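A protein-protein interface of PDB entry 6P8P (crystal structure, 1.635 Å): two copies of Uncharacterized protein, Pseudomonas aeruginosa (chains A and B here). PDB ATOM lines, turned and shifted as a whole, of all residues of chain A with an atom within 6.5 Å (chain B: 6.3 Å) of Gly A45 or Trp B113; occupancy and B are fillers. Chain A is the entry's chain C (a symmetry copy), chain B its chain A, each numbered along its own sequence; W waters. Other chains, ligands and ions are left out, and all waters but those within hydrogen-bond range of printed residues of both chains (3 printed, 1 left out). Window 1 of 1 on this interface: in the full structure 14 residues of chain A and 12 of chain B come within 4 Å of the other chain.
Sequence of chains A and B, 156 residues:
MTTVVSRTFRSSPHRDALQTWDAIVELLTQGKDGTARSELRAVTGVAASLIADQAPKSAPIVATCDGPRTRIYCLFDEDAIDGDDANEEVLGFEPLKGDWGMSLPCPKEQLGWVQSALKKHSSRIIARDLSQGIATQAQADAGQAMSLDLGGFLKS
OG of Ser B49 sits at hydrogen-bond distance from OG of Ser A49. The side-chain amino group (NZ) of Lys B120 sits at hydrogen-bond distance from the backbone carbonyl oxygen (O) of Arg A41, at 3.0 Å. The side-chain hydroxyl of Thr A44 lies within hydrogen-bond range of the side-chain amino group of Lys B120 (3.2 Å).
The side-chain amide nitrogen (NE2) of Gln B110 lies close to the side-chain carboxylate (OD2) of Asp B53, 3.2 Å away. OE1 of Gln B110 is in hydrogen-bond range of NE1 of Trp B113, 3.1 Å away. N of Leu A18 lies within hydrogen-bond range of OD1 of Asp A16, at 2.8 Å. The backbone NH (N) of Gln A19 is in hydrogen-bond range of the side-chain carboxylate (OD1) of Asp A16 (2.8 Å). OG1 of Thr A44 lies within hydrogen-bond range of O of Arg A41 (2.7 Å).
OD1 of Asp A16 touches CB of Trp B113, 3.9 Å away. Trp B113 touches Ala A17. Leu A18 touches Ala B117. Gly A45 touches Trp B113. CG2 of Val A46 touches CA of Gly B45, at 3.97 Å. CB of Ala A48 touches CE3 of Trp B113, 3.5 Å away. Trp B113 touches Ser A49. Ala A52 touches Gln B110 (CB to OE1, 3.7 Å). O of Gly B45 touches CH2 of Trp A113, 3.5 Å away. Ser B49 touches Trp A113.
Gly A45 touches just one residue of chain B: Trp B113. Of the printed residues of chain A, Gln B110 touches Ala A52. Of the printed residues of chain B, Ala A48 touches Trp B113 (3.5 Å). Of the printed residues of chain A, Gly B45 touches Val A46 (3.97 Å) and Trp A113 (3.5 Å). Printed residues of chain B within 4 Å of Asp A16: Trp B113. Val B114 touches none of the printed residues of chain A. Leu B50 touches none of the printed residues of chain A. The nearest residue of chain B that does not touch Gly A45 is Val B46 (4.1 Å). The nearest printed residue of chain B that does not touch Leu A18 is Ser B116 (4.05 Å).
Of the 17 printed residues of chain B, 6 touch a printed residue of chain A. Printed residues of chain B that touch a printed residue of chain A: Gly B45, Ser B49, Gln B110, Trp B113, Ala B117 and Lys B120. Hydrophobic or aromatic side chains of chain B within 4 Å of the printed part of chain A: Trp B113 and Ala B117.
Gly A45 touches Trp B113, and with the chains exchanged Trp A113 touches Gly B45. Val A46 touches Gly B45, but with the chains exchanged Gly A45 does not touch Val B46 (4.1 Å). Ser B49 touches its own counterpart, Ser A49. Ser A49 touches Trp B113, and with the chains exchanged Trp A113 touches Ser B49. 5 positions are printed for both chains. Of the 15 pairs that touch across the chains among the printed residues, 5 have their exchanged pair printed and touching as well.
Water W1 bridges the side-chain carboxylate (OD2) of Asp A16 and the side-chain hydroxyl (OG) of Ser B116. Water W3 lies within hydrogen-bond range of a ring nitrogen (NE2) of His B121 (3.0 Å), the backbone NH of Gly A45 (3.2 Å) and the backbone carbonyl oxygen of Ala A42 (3.4 Å). Water W2 lies within hydrogen-bond range of NE2 of His B121, O of Ala B117 and N of Gly A45.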
ATOM      1  N   ASP A  16       1.465 -32.961 -16.156  1.00  0.00           N
ATOM      2  CA  ASP A  16       2.843 -33.258 -15.789  1.00  0.00           C
ATOM      3  C   ASP A  16       3.195 -32.468 -14.525  1.00  0.00           C
ATOM      4  O   ASP A  16       2.429 -31.618 -14.051  1.00  0.00           O
ATOM      5  CB  ASP A  16       3.792 -32.998 -16.973  1.00  0.00           C
ATOM      6  CG  ASP A  16       4.017 -31.533 -17.287  1.00  0.00           C
ATOM      7  OD1 ASP A  16       4.198 -30.704 -16.379  1.00  0.00           O
ATOM      8  OD2 ASP A  16       4.108 -31.208 -18.491  1.00  0.00           O
ATOM      9  N   ALA A  17       4.369 -32.752 -13.966  1.00  0.00           N
ATOM     10  CA  ALA A  17       4.684 -32.192 -12.652  1.00  0.00           C
ATOM     11  C   ALA A  17       4.742 -30.671 -12.673  1.00  0.00           C
ATOM     12  O   ALA A  17       4.361 -30.018 -11.695  1.00  0.00           O
ATOM     13  CB  ALA A  17       5.995 -32.781 -12.141  1.00  0.00           C
ATOM     14  N   LEU A  18       5.177 -30.086 -13.784  1.00  0.00           N
ATOM     15  CA  LEU A  18       5.266 -28.637 -13.875  1.00  0.00           C
ATOM     16  C   LEU A  18       3.887 -28.019 -14.048  1.00  0.00           C
ATOM     17  O   LEU A  18       3.572 -27.010 -13.406  1.00  0.00           O
ATOM     18  CB  LEU A  18       6.175 -28.231 -15.038  1.00  0.00           C
ATOM     19  CG  LEU A  18       6.296 -26.729 -15.221  1.00  0.00           C
ATOM     20  CD1 LEU A  18       7.767 -26.328 -15.346  1.00  0.00           C
ATOM     21  CD2 LEU A  18       5.520 -26.296 -16.450  1.00  0.00           C
ATOM     22  N   GLN A  19       3.064 -28.594 -14.931  1.00  0.00           N
ATOM     23  CA  GLN A  19       1.676 -28.150 -15.048  1.00  0.00           C
ATOM     24  C   GLN A  19       0.945 -28.241 -13.713  1.00  0.00           C
ATOM     25  O   GLN A  19       0.052 -27.433 -13.443  1.00  0.00           O
ATOM     26  CB  GLN A  19       0.960 -28.991 -16.098  1.00  0.00           C
ATOM     27  CG  GLN A  19       1.595 -28.902 -17.502  1.00  0.00           C
ATOM     28  CD  GLN A  19       0.997 -29.916 -18.491  1.00  0.00           C
ATOM     29  OE1 GLN A  19       0.654 -31.045 -18.127  1.00  0.00           O
ATOM     30  NE2 GLN A  19       0.890 -29.512 -19.741  1.00  0.00           N
ATOM     31  N   TRP A  21       2.365 -27.913 -10.624  1.00  0.00           N
ATOM     32  CA  TRP A  21       2.790 -26.757  -9.843  1.00  0.00           C
ATOM     33  C   TRP A  21       2.110 -25.488 -10.335  1.00  0.00           C
ATOM     34  O   TRP A  21       1.616 -24.683  -9.539  1.00  0.00           O
ATOM     35  CB  TRP A  21       4.303 -26.606  -9.904  1.00  0.00           C
ATOM     36  CG  TRP A  21       4.827 -25.484  -9.092  1.00  0.00           C
ATOM     37  CD1 TRP A  21       5.512 -24.387  -9.552  1.00  0.00           C
ATOM     38  CD2 TRP A  21       4.708 -25.314  -7.679  1.00  0.00           C
ATOM     39  NE1 TRP A  21       5.843 -23.569  -8.511  1.00  0.00           N
ATOM     40  CE2 TRP A  21       5.367 -24.115  -7.345  1.00  0.00           C
ATOM     41  CE3 TRP A  21       4.120 -26.061  -6.659  1.00  0.00           C
ATOM     42  CZ2 TRP A  21       5.463 -23.658  -6.032  1.00  0.00           C
ATOM     43  CZ3 TRP A  21       4.214 -25.597  -5.352  1.00  0.00           C
ATOM     44  CH2 TRP A  21       4.868 -24.405  -5.055  1.00  0.00           C
ATOM     45  N   ARG A  41       6.792 -19.021  -8.438  1.00  0.00           N
ATOM     46  CA  ARG A  41       7.246 -19.365  -9.774  1.00  0.00           C
ATOM     47  C   ARG A  41       8.753 -19.578  -9.786  1.00  0.00           C
ATOM     48  O   ARG A  41       9.250 -20.448 -10.519  1.00  0.00           O
ATOM     49  CB  ARG A  41       6.810 -18.296 -10.780  1.00  0.00           C
ATOM     50  CG  ARG A  41       5.299 -18.353 -11.104  1.00  0.00           C
ATOM     51  CD  ARG A  41       4.918 -17.294 -12.118  1.00  0.00           C
ATOM     52  NE  ARG A  41       5.612 -17.483 -13.392  1.00  0.00           N
ATOM     53  CZ  ARG A  41       5.172 -18.271 -14.369  1.00  0.00           C
ATOM     54  NH1 ARG A  41       4.039 -18.941 -14.217  1.00  0.00           N
ATOM     55  NH2 ARG A  41       5.861 -18.387 -15.495  1.00  0.00           N
ATOM     56  N   ALA A  42       9.478 -18.867  -8.917  1.00  0.00           N
ATOM     57  CA  ALA A  42      10.938 -18.988  -8.886  1.00  0.00           C
ATOM     58  C   ALA A  42      11.419 -20.367  -8.438  1.00  0.00           C
ATOM     59  O   ALA A  42      12.521 -20.782  -8.825  1.00  0.00           O
ATOM     60  CB  ALA A  42      11.526 -17.918  -7.976  1.00  0.00           C
ATOM     61  N   VAL A  43      10.622 -21.098  -7.656  1.00  0.00           N
ATOM     62  CA  VAL A  43      11.022 -22.419  -7.181  1.00  0.00           C
ATOM     63  C   VAL A  43      10.406 -23.535  -8.027  1.00  0.00           C
ATOM     64  O   VAL A  43      10.407 -24.709  -7.612  1.00  0.00           O
ATOM     65  CB  VAL A  43      10.693 -22.618  -5.691  1.00  0.00           C
ATOM     66  CG1 VAL A  43      11.372 -21.565  -4.860  1.00  0.00           C
ATOM     67  CG2 VAL A  43       9.174 -22.649  -5.488  1.00  0.00           C
ATOM     68  N   THR A  44       9.958 -23.213  -9.248  1.00  0.00           N
ATOM     69  CA  THR A  44       9.225 -24.195 -10.047  1.00  0.00           C
ATOM     70  C   THR A  44      10.018 -25.478 -10.247  1.00  0.00           C
ATOM     71  O   THR A  44       9.465 -26.573 -10.105  1.00  0.00           O
ATOM     72  CB  THR A  44       8.848 -23.603 -11.406  1.00  0.00           C
ATOM     73  OG1 THR A  44       7.833 -22.596 -11.228  1.00  0.00           O
ATOM     74  CG2 THR A  44       8.303 -24.692 -12.342  1.00  0.00           C
ATOM     75  N   GLY A  45      11.312 -25.365 -10.571  1.00  0.00           N
ATOM     76  CA  GLY A  45      12.124 -26.560 -10.786  1.00  0.00           C
ATOM     77  C   GLY A  45      12.154 -27.501  -9.592  1.00  0.00           C
ATOM     78  O   GLY A  45      12.016 -28.720  -9.736  1.00  0.00           O
ATOM     79  N   VAL A  46      12.353 -26.952  -8.402  1.00  0.00           N
ATOM     80  CA  VAL A  46      12.367 -27.770  -7.194  1.00  0.00           C
ATOM     81  C   VAL A  46      10.974 -28.343  -6.909  1.00  0.00           C
ATOM     82  O   VAL A  46      10.809 -29.542  -6.651  1.00  0.00           O
ATOM     83  CB  VAL A  46      12.882 -26.942  -6.003  1.00  0.00           C
ATOM     84  CG1 VAL A  46      12.968 -27.835  -4.772  1.00  0.00           C
ATOM     85  CG2 VAL A  46      14.213 -26.331  -6.316  1.00  0.00           C
ATOM     86  N   ALA A  47       9.955 -27.493  -6.968  1.00  0.00           N
ATOM     87  CA  ALA A  47       8.586 -27.924  -6.649  1.00  0.00           C
ATOM     88  C   ALA A  47       8.128 -29.026  -7.598  1.00  0.00           C
ATOM     89  O   ALA A  47       7.556 -30.041  -7.166  1.00  0.00           O
ATOM     90  CB  ALA A  47       7.633 -26.734  -6.728  1.00  0.00           C
ATOM     91  N   ALA A  48       8.395 -28.849  -8.897  1.00  0.00           N
ATOM     92  CA  ALA A  48       8.040 -29.867  -9.882  1.00  0.00           C
ATOM     93  C   ALA A  48       8.790 -31.175  -9.641  1.00  0.00           C
ATOM     94  O   ALA A  48       8.214 -32.264  -9.761  1.00  0.00           O
ATOM     95  CB  ALA A  48       8.303 -29.341 -11.293  1.00  0.00           C
ATOM     96  N   SER A  49      10.053 -31.088  -9.249  1.00  0.00           N
ATOM     97  CA  SER A  49      10.808 -32.291  -8.929  1.00  0.00           C
ATOM     98  C   SER A  49      10.138 -33.058  -7.815  1.00  0.00           C
ATOM     99  O   SER A  49      10.057 -34.287  -7.860  1.00  0.00           O
ATOM    100  CB  SER A  49      12.225 -31.915  -8.506  1.00  0.00           C
ATOM    101  OG  SER A  49      12.992 -33.060  -8.200  1.00  0.00           O
ATOM    102  N   LEU A  50       9.649 -32.330  -6.805  1.00  0.00           N
ATOM    103  CA  LEU A  50       9.004 -32.977  -5.670  1.00  0.00           C
ATOM    104  C   LEU A  50       7.689 -33.613  -6.075  1.00  0.00           C
ATOM    105  O   LEU A  50       7.369 -34.733  -5.657  1.00  0.00           O
ATOM    106  CB  LEU A  50       8.772 -31.958  -4.570  1.00  0.00           C
ATOM    107  CG  LEU A  50      10.033 -31.325  -3.976  1.00  0.00           C
ATOM    108  CD1 LEU A  50       9.776 -30.269  -2.918  1.00  0.00           C
ATOM    109  CD2 LEU A  50      10.940 -32.422  -3.352  1.00  0.00           C
ATOM    110  N   ALA A  52       6.974 -34.684  -9.082  1.00  0.00           N
ATOM    111  CA  ALA A  52       7.300 -35.860  -9.890  1.00  0.00           C
ATOM    112  C   ALA A  52       7.667 -37.051  -9.019  1.00  0.00           C
ATOM    113  O   ALA A  52       7.455 -38.202  -9.409  1.00  0.00           O
ATOM    114  CB  ALA A  52       8.426 -35.538 -10.881  1.00  0.00           C
ATOM    115  N   TRP A 113      19.616 -31.396  -0.689  1.00  0.00           N
ATOM    116  CA  TRP A 113      19.725 -30.554  -1.875  1.00  0.00           C
ATOM    117  C   TRP A 113      18.511 -29.642  -2.019  1.00  0.00           C
ATOM    118  O   TRP A 113      18.645 -28.468  -2.390  1.00  0.00           O
ATOM    119  CB  TRP A 113      19.937 -31.418  -3.126  1.00  0.00           C
ATOM    120  CG  TRP A 113      18.759 -32.007  -3.847  1.00  0.00           C
ATOM    121  CD1 TRP A 113      18.342 -33.308  -3.814  1.00  0.00           C
ATOM    122  CD2 TRP A 113      17.891 -31.337  -4.776  1.00  0.00           C
ATOM    123  NE1 TRP A 113      17.240 -33.480  -4.642  1.00  0.00           N
ATOM    124  CE2 TRP A 113      16.959 -32.289  -5.251  1.00  0.00           C
ATOM    125  CE3 TRP A 113      17.776 -30.012  -5.210  1.00  0.00           C
ATOM    126  CZ2 TRP A 113      15.925 -31.953  -6.127  1.00  0.00           C
ATOM    127  CZ3 TRP A 113      16.775 -29.688  -6.122  1.00  0.00           C
ATOM    128  CH2 TRP A 113      15.855 -30.652  -6.568  1.00  0.00           C
ATOM    129  N   GLY B  45      17.636 -26.137  -9.910  1.00  0.00           N
ATOM    130  CA  GLY B  45      16.606 -27.034  -9.401  1.00  0.00           C
ATOM    131  C   GLY B  45      16.411 -28.246 -10.300  1.00  0.00           C
ATOM    132  O   GLY B  45      16.345 -29.394  -9.837  1.00  0.00           O
ATOM    133  N   VAL B  46      16.323 -28.004 -11.603  1.00  0.00           N
ATOM    134  CA  VAL B  46      16.134 -29.094 -12.551  1.00  0.00           C
ATOM    135  C   VAL B  46      17.377 -29.977 -12.582  1.00  0.00           C
ATOM    136  O   VAL B  46      17.298 -31.213 -12.532  1.00  0.00           O
ATOM    137  CB  VAL B  46      15.795 -28.537 -13.951  1.00  0.00           C
ATOM    138  CG1 VAL B  46      15.727 -29.664 -14.955  1.00  0.00           C
ATOM    139  CG2 VAL B  46      14.508 -27.754 -13.910  1.00  0.00           C
ATOM    140  N   SER B  49      17.790 -32.059  -9.582  1.00  0.00           N
ATOM    141  CA  SER B  49      16.794 -33.123  -9.578  1.00  0.00           C
ATOM    142  C   SER B  49      17.254 -34.318 -10.396  1.00  0.00           C
ATOM    143  O   SER B  49      17.111 -35.470  -9.968  1.00  0.00           O
ATOM    144  CB  SER B  49      15.465 -32.586 -10.133  1.00  0.00           C
ATOM    145  OG  SER B  49      14.454 -33.597 -10.227  1.00  0.00           O
ATOM    146  N   LEU B  50      17.812 -34.051 -11.570  1.00  0.00           N
ATOM    147  CA  LEU B  50      18.270 -35.118 -12.450  1.00  0.00           C
ATOM    148  C   LEU B  50      19.468 -35.848 -11.857  1.00  0.00           C
ATOM    149  O   LEU B  50      19.592 -37.065 -11.995  1.00  0.00           O
ATOM    150  CB  LEU B  50      18.632 -34.533 -13.822  1.00  0.00           C
ATOM    151  CG  LEU B  50      17.477 -33.945 -14.615  1.00  0.00           C
ATOM    152  CD1 LEU B  50      18.015 -33.147 -15.808  1.00  0.00           C
ATOM    153  CD2 LEU B  50      16.517 -35.022 -15.048  1.00  0.00           C
ATOM    154  N   ASP B  53      18.386 -38.244  -9.301  1.00  0.00           N
ATOM    155  CA  ASP B  53      17.853 -39.438  -9.946  1.00  0.00           C
ATOM    156  C   ASP B  53      18.924 -40.246 -10.670  1.00  0.00           C
ATOM    157  O   ASP B  53      18.584 -41.234 -11.331  1.00  0.00           O
ATOM    158  CB  ASP B  53      16.726 -39.040 -10.904  1.00  0.00           C
ATOM    159  CG  ASP B  53      15.429 -38.631 -10.138  1.00  0.00           C
ATOM    160  OD1 ASP B  53      15.170 -39.210  -9.064  1.00  0.00           O
ATOM    161  OD2 ASP B  53      14.681 -37.736 -10.605  1.00  0.00           O
ATOM    162  N   GLU B 109      10.444 -40.575 -19.068  1.00  0.00           N
ATOM    163  CA  GLU B 109       9.154 -40.295 -18.443  1.00  0.00           C
ATOM    164  C   GLU B 109       9.105 -38.919 -17.790  1.00  0.00           C
ATOM    165  O   GLU B 109       8.011 -38.387 -17.572  1.00  0.00           O
ATOM    166  CB  GLU B 109       8.807 -41.366 -17.397  1.00  0.00           C
ATOM    167  CG  GLU B 109       9.706 -41.432 -16.177  1.00  0.00           C
ATOM    168  CD  GLU B 109       9.020 -42.131 -14.995  1.00  0.00           C
ATOM    169  OE1 GLU B 109       9.716 -42.757 -14.164  1.00  0.00           O
ATOM    170  OE2 GLU B 109       7.775 -42.054 -14.896  1.00  0.00           O
ATOM    171  N   GLN B 110      10.256 -38.332 -17.463  1.00  0.00           N
ATOM    172  CA  GLN B 110      10.292 -36.999 -16.874  1.00  0.00           C
ATOM    173  C   GLN B 110      10.567 -35.907 -17.898  1.00  0.00           C
ATOM    174  O   GLN B 110      10.621 -34.738 -17.535  1.00  0.00           O
ATOM    175  CB  GLN B 110      11.330 -36.964 -15.752  1.00  0.00           C
ATOM    176  CG  GLN B 110      10.967 -37.899 -14.569  1.00  0.00           C
ATOM    177  CD  GLN B 110      11.768 -37.623 -13.305  1.00  0.00           C
ATOM    178  OE1 GLN B 110      11.514 -36.650 -12.571  1.00  0.00           O
ATOM    179  NE2 GLN B 110      12.742 -38.487 -13.038  1.00  0.00           N
ATOM    180  N   LEU B 111      10.733 -36.249 -19.174  1.00  0.00           N
ATOM    181  CA  LEU B 111      11.182 -35.240 -20.119  1.00  0.00           C
ATOM    182  C   LEU B 111      10.168 -34.119 -20.258  1.00  0.00           C
ATOM    183  O   LEU B 111      10.531 -32.967 -20.516  1.00  0.00           O
ATOM    184  CB  LEU B 111      11.420 -35.855 -21.500  1.00  0.00           C
ATOM    185  CG  LEU B 111      12.793 -36.320 -21.876  1.00  0.00           C
ATOM    186  CD1 LEU B 111      12.722 -36.858 -23.350  1.00  0.00           C
ATOM    187  CD2 LEU B 111      13.822 -35.247 -21.729  1.00  0.00           C
ATOM    188  N   GLY B 112       8.887 -34.446 -20.173  1.00  0.00           N
ATOM    189  CA  GLY B 112       7.853 -33.439 -20.326  1.00  0.00           C
ATOM    190  C   GLY B 112       8.035 -32.285 -19.367  1.00  0.00           C
ATOM    191  O   GLY B 112       8.145 -31.124 -19.778  1.00  0.00           O
ATOM    192  N   TRP B 113       8.102 -32.585 -18.070  1.00  0.00           N
ATOM    193  CA  TRP B 113       8.235 -31.503 -17.104  1.00  0.00           C
ATOM    194  C   TRP B 113       9.630 -30.894 -17.150  1.00  0.00           C
ATOM    195  O   TRP B 113       9.777 -29.673 -17.039  1.00  0.00           O
ATOM    196  CB  TRP B 113       7.855 -31.983 -15.697  1.00  0.00           C
ATOM    197  CG  TRP B 113       8.899 -32.621 -14.821  1.00  0.00           C
ATOM    198  CD1 TRP B 113       9.038 -33.958 -14.538  1.00  0.00           C
ATOM    199  CD2 TRP B 113       9.895 -31.939 -14.048  1.00  0.00           C
ATOM    200  NE1 TRP B 113      10.087 -34.136 -13.660  1.00  0.00           N
ATOM    201  CE2 TRP B 113      10.627 -32.915 -13.352  1.00  0.00           C
ATOM    202  CE3 TRP B 113      10.257 -30.596 -13.903  1.00  0.00           C
ATOM    203  CZ2 TRP B 113      11.682 -32.588 -12.496  1.00  0.00           C
ATOM    204  CZ3 TRP B 113      11.282 -30.282 -13.051  1.00  0.00           C
ATOM    205  CH2 TRP B 113      11.999 -31.271 -12.380  1.00  0.00           C
ATOM    206  N   VAL B 114      10.652 -31.714 -17.376  1.00  0.00           N
ATOM    207  CA  VAL B 114      12.014 -31.191 -17.347  1.00  0.00           C
ATOM    208  C   VAL B 114      12.247 -30.231 -18.497  1.00  0.00           C
ATOM    209  O   VAL B 114      12.853 -29.177 -18.310  1.00  0.00           O
ATOM    210  CB  VAL B 114      13.012 -32.354 -17.342  1.00  0.00           C
ATOM    211  CG1 VAL B 114      14.411 -31.842 -17.627  1.00  0.00           C
ATOM    212  CG2 VAL B 114      12.953 -33.044 -16.010  1.00  0.00           C
ATOM    213  N   GLN B 115      11.825 -30.588 -19.714  1.00  0.00           N
ATOM    214  CA  GLN B 115      12.079 -29.705 -20.847  1.00  0.00           C
ATOM    215  C   GLN B 115      11.339 -28.385 -20.687  1.00  0.00           C
ATOM    216  O   GLN B 115      11.893 -27.321 -20.984  1.00  0.00           O
ATOM    217  CB  GLN B 115      11.708 -30.400 -22.163  1.00  0.00           C
ATOM    218  CG  GLN B 115      12.610 -31.606 -22.443  1.00  0.00           C
ATOM    219  CD  GLN B 115      12.407 -32.232 -23.812  1.00  0.00           C
ATOM    220  OE1 GLN B 115      13.368 -32.640 -24.491  1.00  0.00           O
ATOM    221  NE2 GLN B 115      11.160 -32.331 -24.221  1.00  0.00           N
ATOM    222  N   SER B 116      10.104 -28.430 -20.161  1.00  0.00           N
ATOM    223  CA  SER B 116       9.375 -27.194 -19.888  1.00  0.00           C
ATOM    224  C   SER B 116      10.063 -26.353 -18.824  1.00  0.00           C
ATOM    225  O   SER B 116      10.129 -25.129 -18.945  1.00  0.00           O
ATOM    226  CB  SER B 116       7.937 -27.511 -19.461  1.00  0.00           C
ATOM    227  OG  SER B 116       7.215 -28.071 -20.526  1.00  0.00           O
ATOM    228  N   ALA B 117      10.533 -26.980 -17.750  1.00  0.00           N
ATOM    229  CA  ALA B 117      11.218 -26.255 -16.690  1.00  0.00           C
ATOM    230  C   ALA B 117      12.489 -25.602 -17.198  1.00  0.00           C
ATOM    231  O   ALA B 117      12.822 -24.486 -16.789  1.00  0.00           O
ATOM    232  CB  ALA B 117      11.525 -27.194 -15.528  1.00  0.00           C
ATOM    233  N   LEU B 118      13.237 -26.291 -18.058  1.00  0.00           N
ATOM    234  CA  LEU B 118      14.456 -25.696 -18.586  1.00  0.00           C
ATOM    235  C   LEU B 118      14.144 -24.516 -19.492  1.00  0.00           C
ATOM    236  O   LEU B 118      14.866 -23.509 -19.485  1.00  0.00           O
ATOM    237  CB  LEU B 118      15.255 -26.740 -19.362  1.00  0.00           C
ATOM    238  CG  LEU B 118      15.924 -27.796 -18.520  1.00  0.00           C
ATOM    239  CD1 LEU B 118      16.641 -28.840 -19.401  1.00  0.00           C
ATOM    240  CD2 LEU B 118      16.962 -27.213 -17.557  1.00  0.00           C
ATOM    241  N   LYS B 120      12.086 -22.311 -19.337  1.00  0.00           N
ATOM    242  CA  LYS B 120      11.839 -21.061 -18.636  1.00  0.00           C
ATOM    243  C   LYS B 120      13.107 -20.231 -18.501  1.00  0.00           C
ATOM    244  O   LYS B 120      13.035 -19.004 -18.400  1.00  0.00           O
ATOM    245  CB  LYS B 120      11.295 -21.325 -17.227  1.00  0.00           C
ATOM    246  CG  LYS B 120      10.029 -22.145 -17.118  1.00  0.00           C
ATOM    247  CD  LYS B 120       9.543 -22.194 -15.645  1.00  0.00           C
ATOM    248  CE  LYS B 120       9.839 -20.891 -14.877  1.00  0.00           C
ATOM    249  NZ  LYS B 120       9.446 -20.879 -13.442  1.00  0.00           N
ATOM    250  N   HIS B 121      14.275 -20.884 -18.447  1.00  0.00           N
ATOM    251  CA  HIS B 121      15.504 -20.208 -18.096  1.00  0.00           C
ATOM    252  C   HIS B 121      16.501 -20.102 -19.235  1.00  0.00           C
ATOM    253  O   HIS B 121      17.431 -19.300 -19.136  1.00  0.00           O
ATOM    254  CB  HIS B 121      16.227 -20.938 -16.947  1.00  0.00           C
ATOM    255  CG  HIS B 121      15.394 -21.116 -15.726  1.00  0.00           C
ATOM    256  ND1 HIS B 121      15.056 -20.065 -14.906  1.00  0.00           N
ATOM    257  CD2 HIS B 121      14.861 -22.227 -15.158  1.00  0.00           C
ATOM    258  CE1 HIS B 121      14.309 -20.511 -13.909  1.00  0.00           C
ATOM    259  NE2 HIS B 121      14.184 -21.822 -14.034  1.00  0.00           N
HETATM  260  O   HOH W   1       4.954 -28.923 -19.349  1.00  0.00           O
HETATM  261  O   HOH W   2      12.785 -24.422 -13.500  1.00  0.00           O
HETATM  262  O   HOH W   3      12.519 -22.653 -11.693  1.00  0.00           O
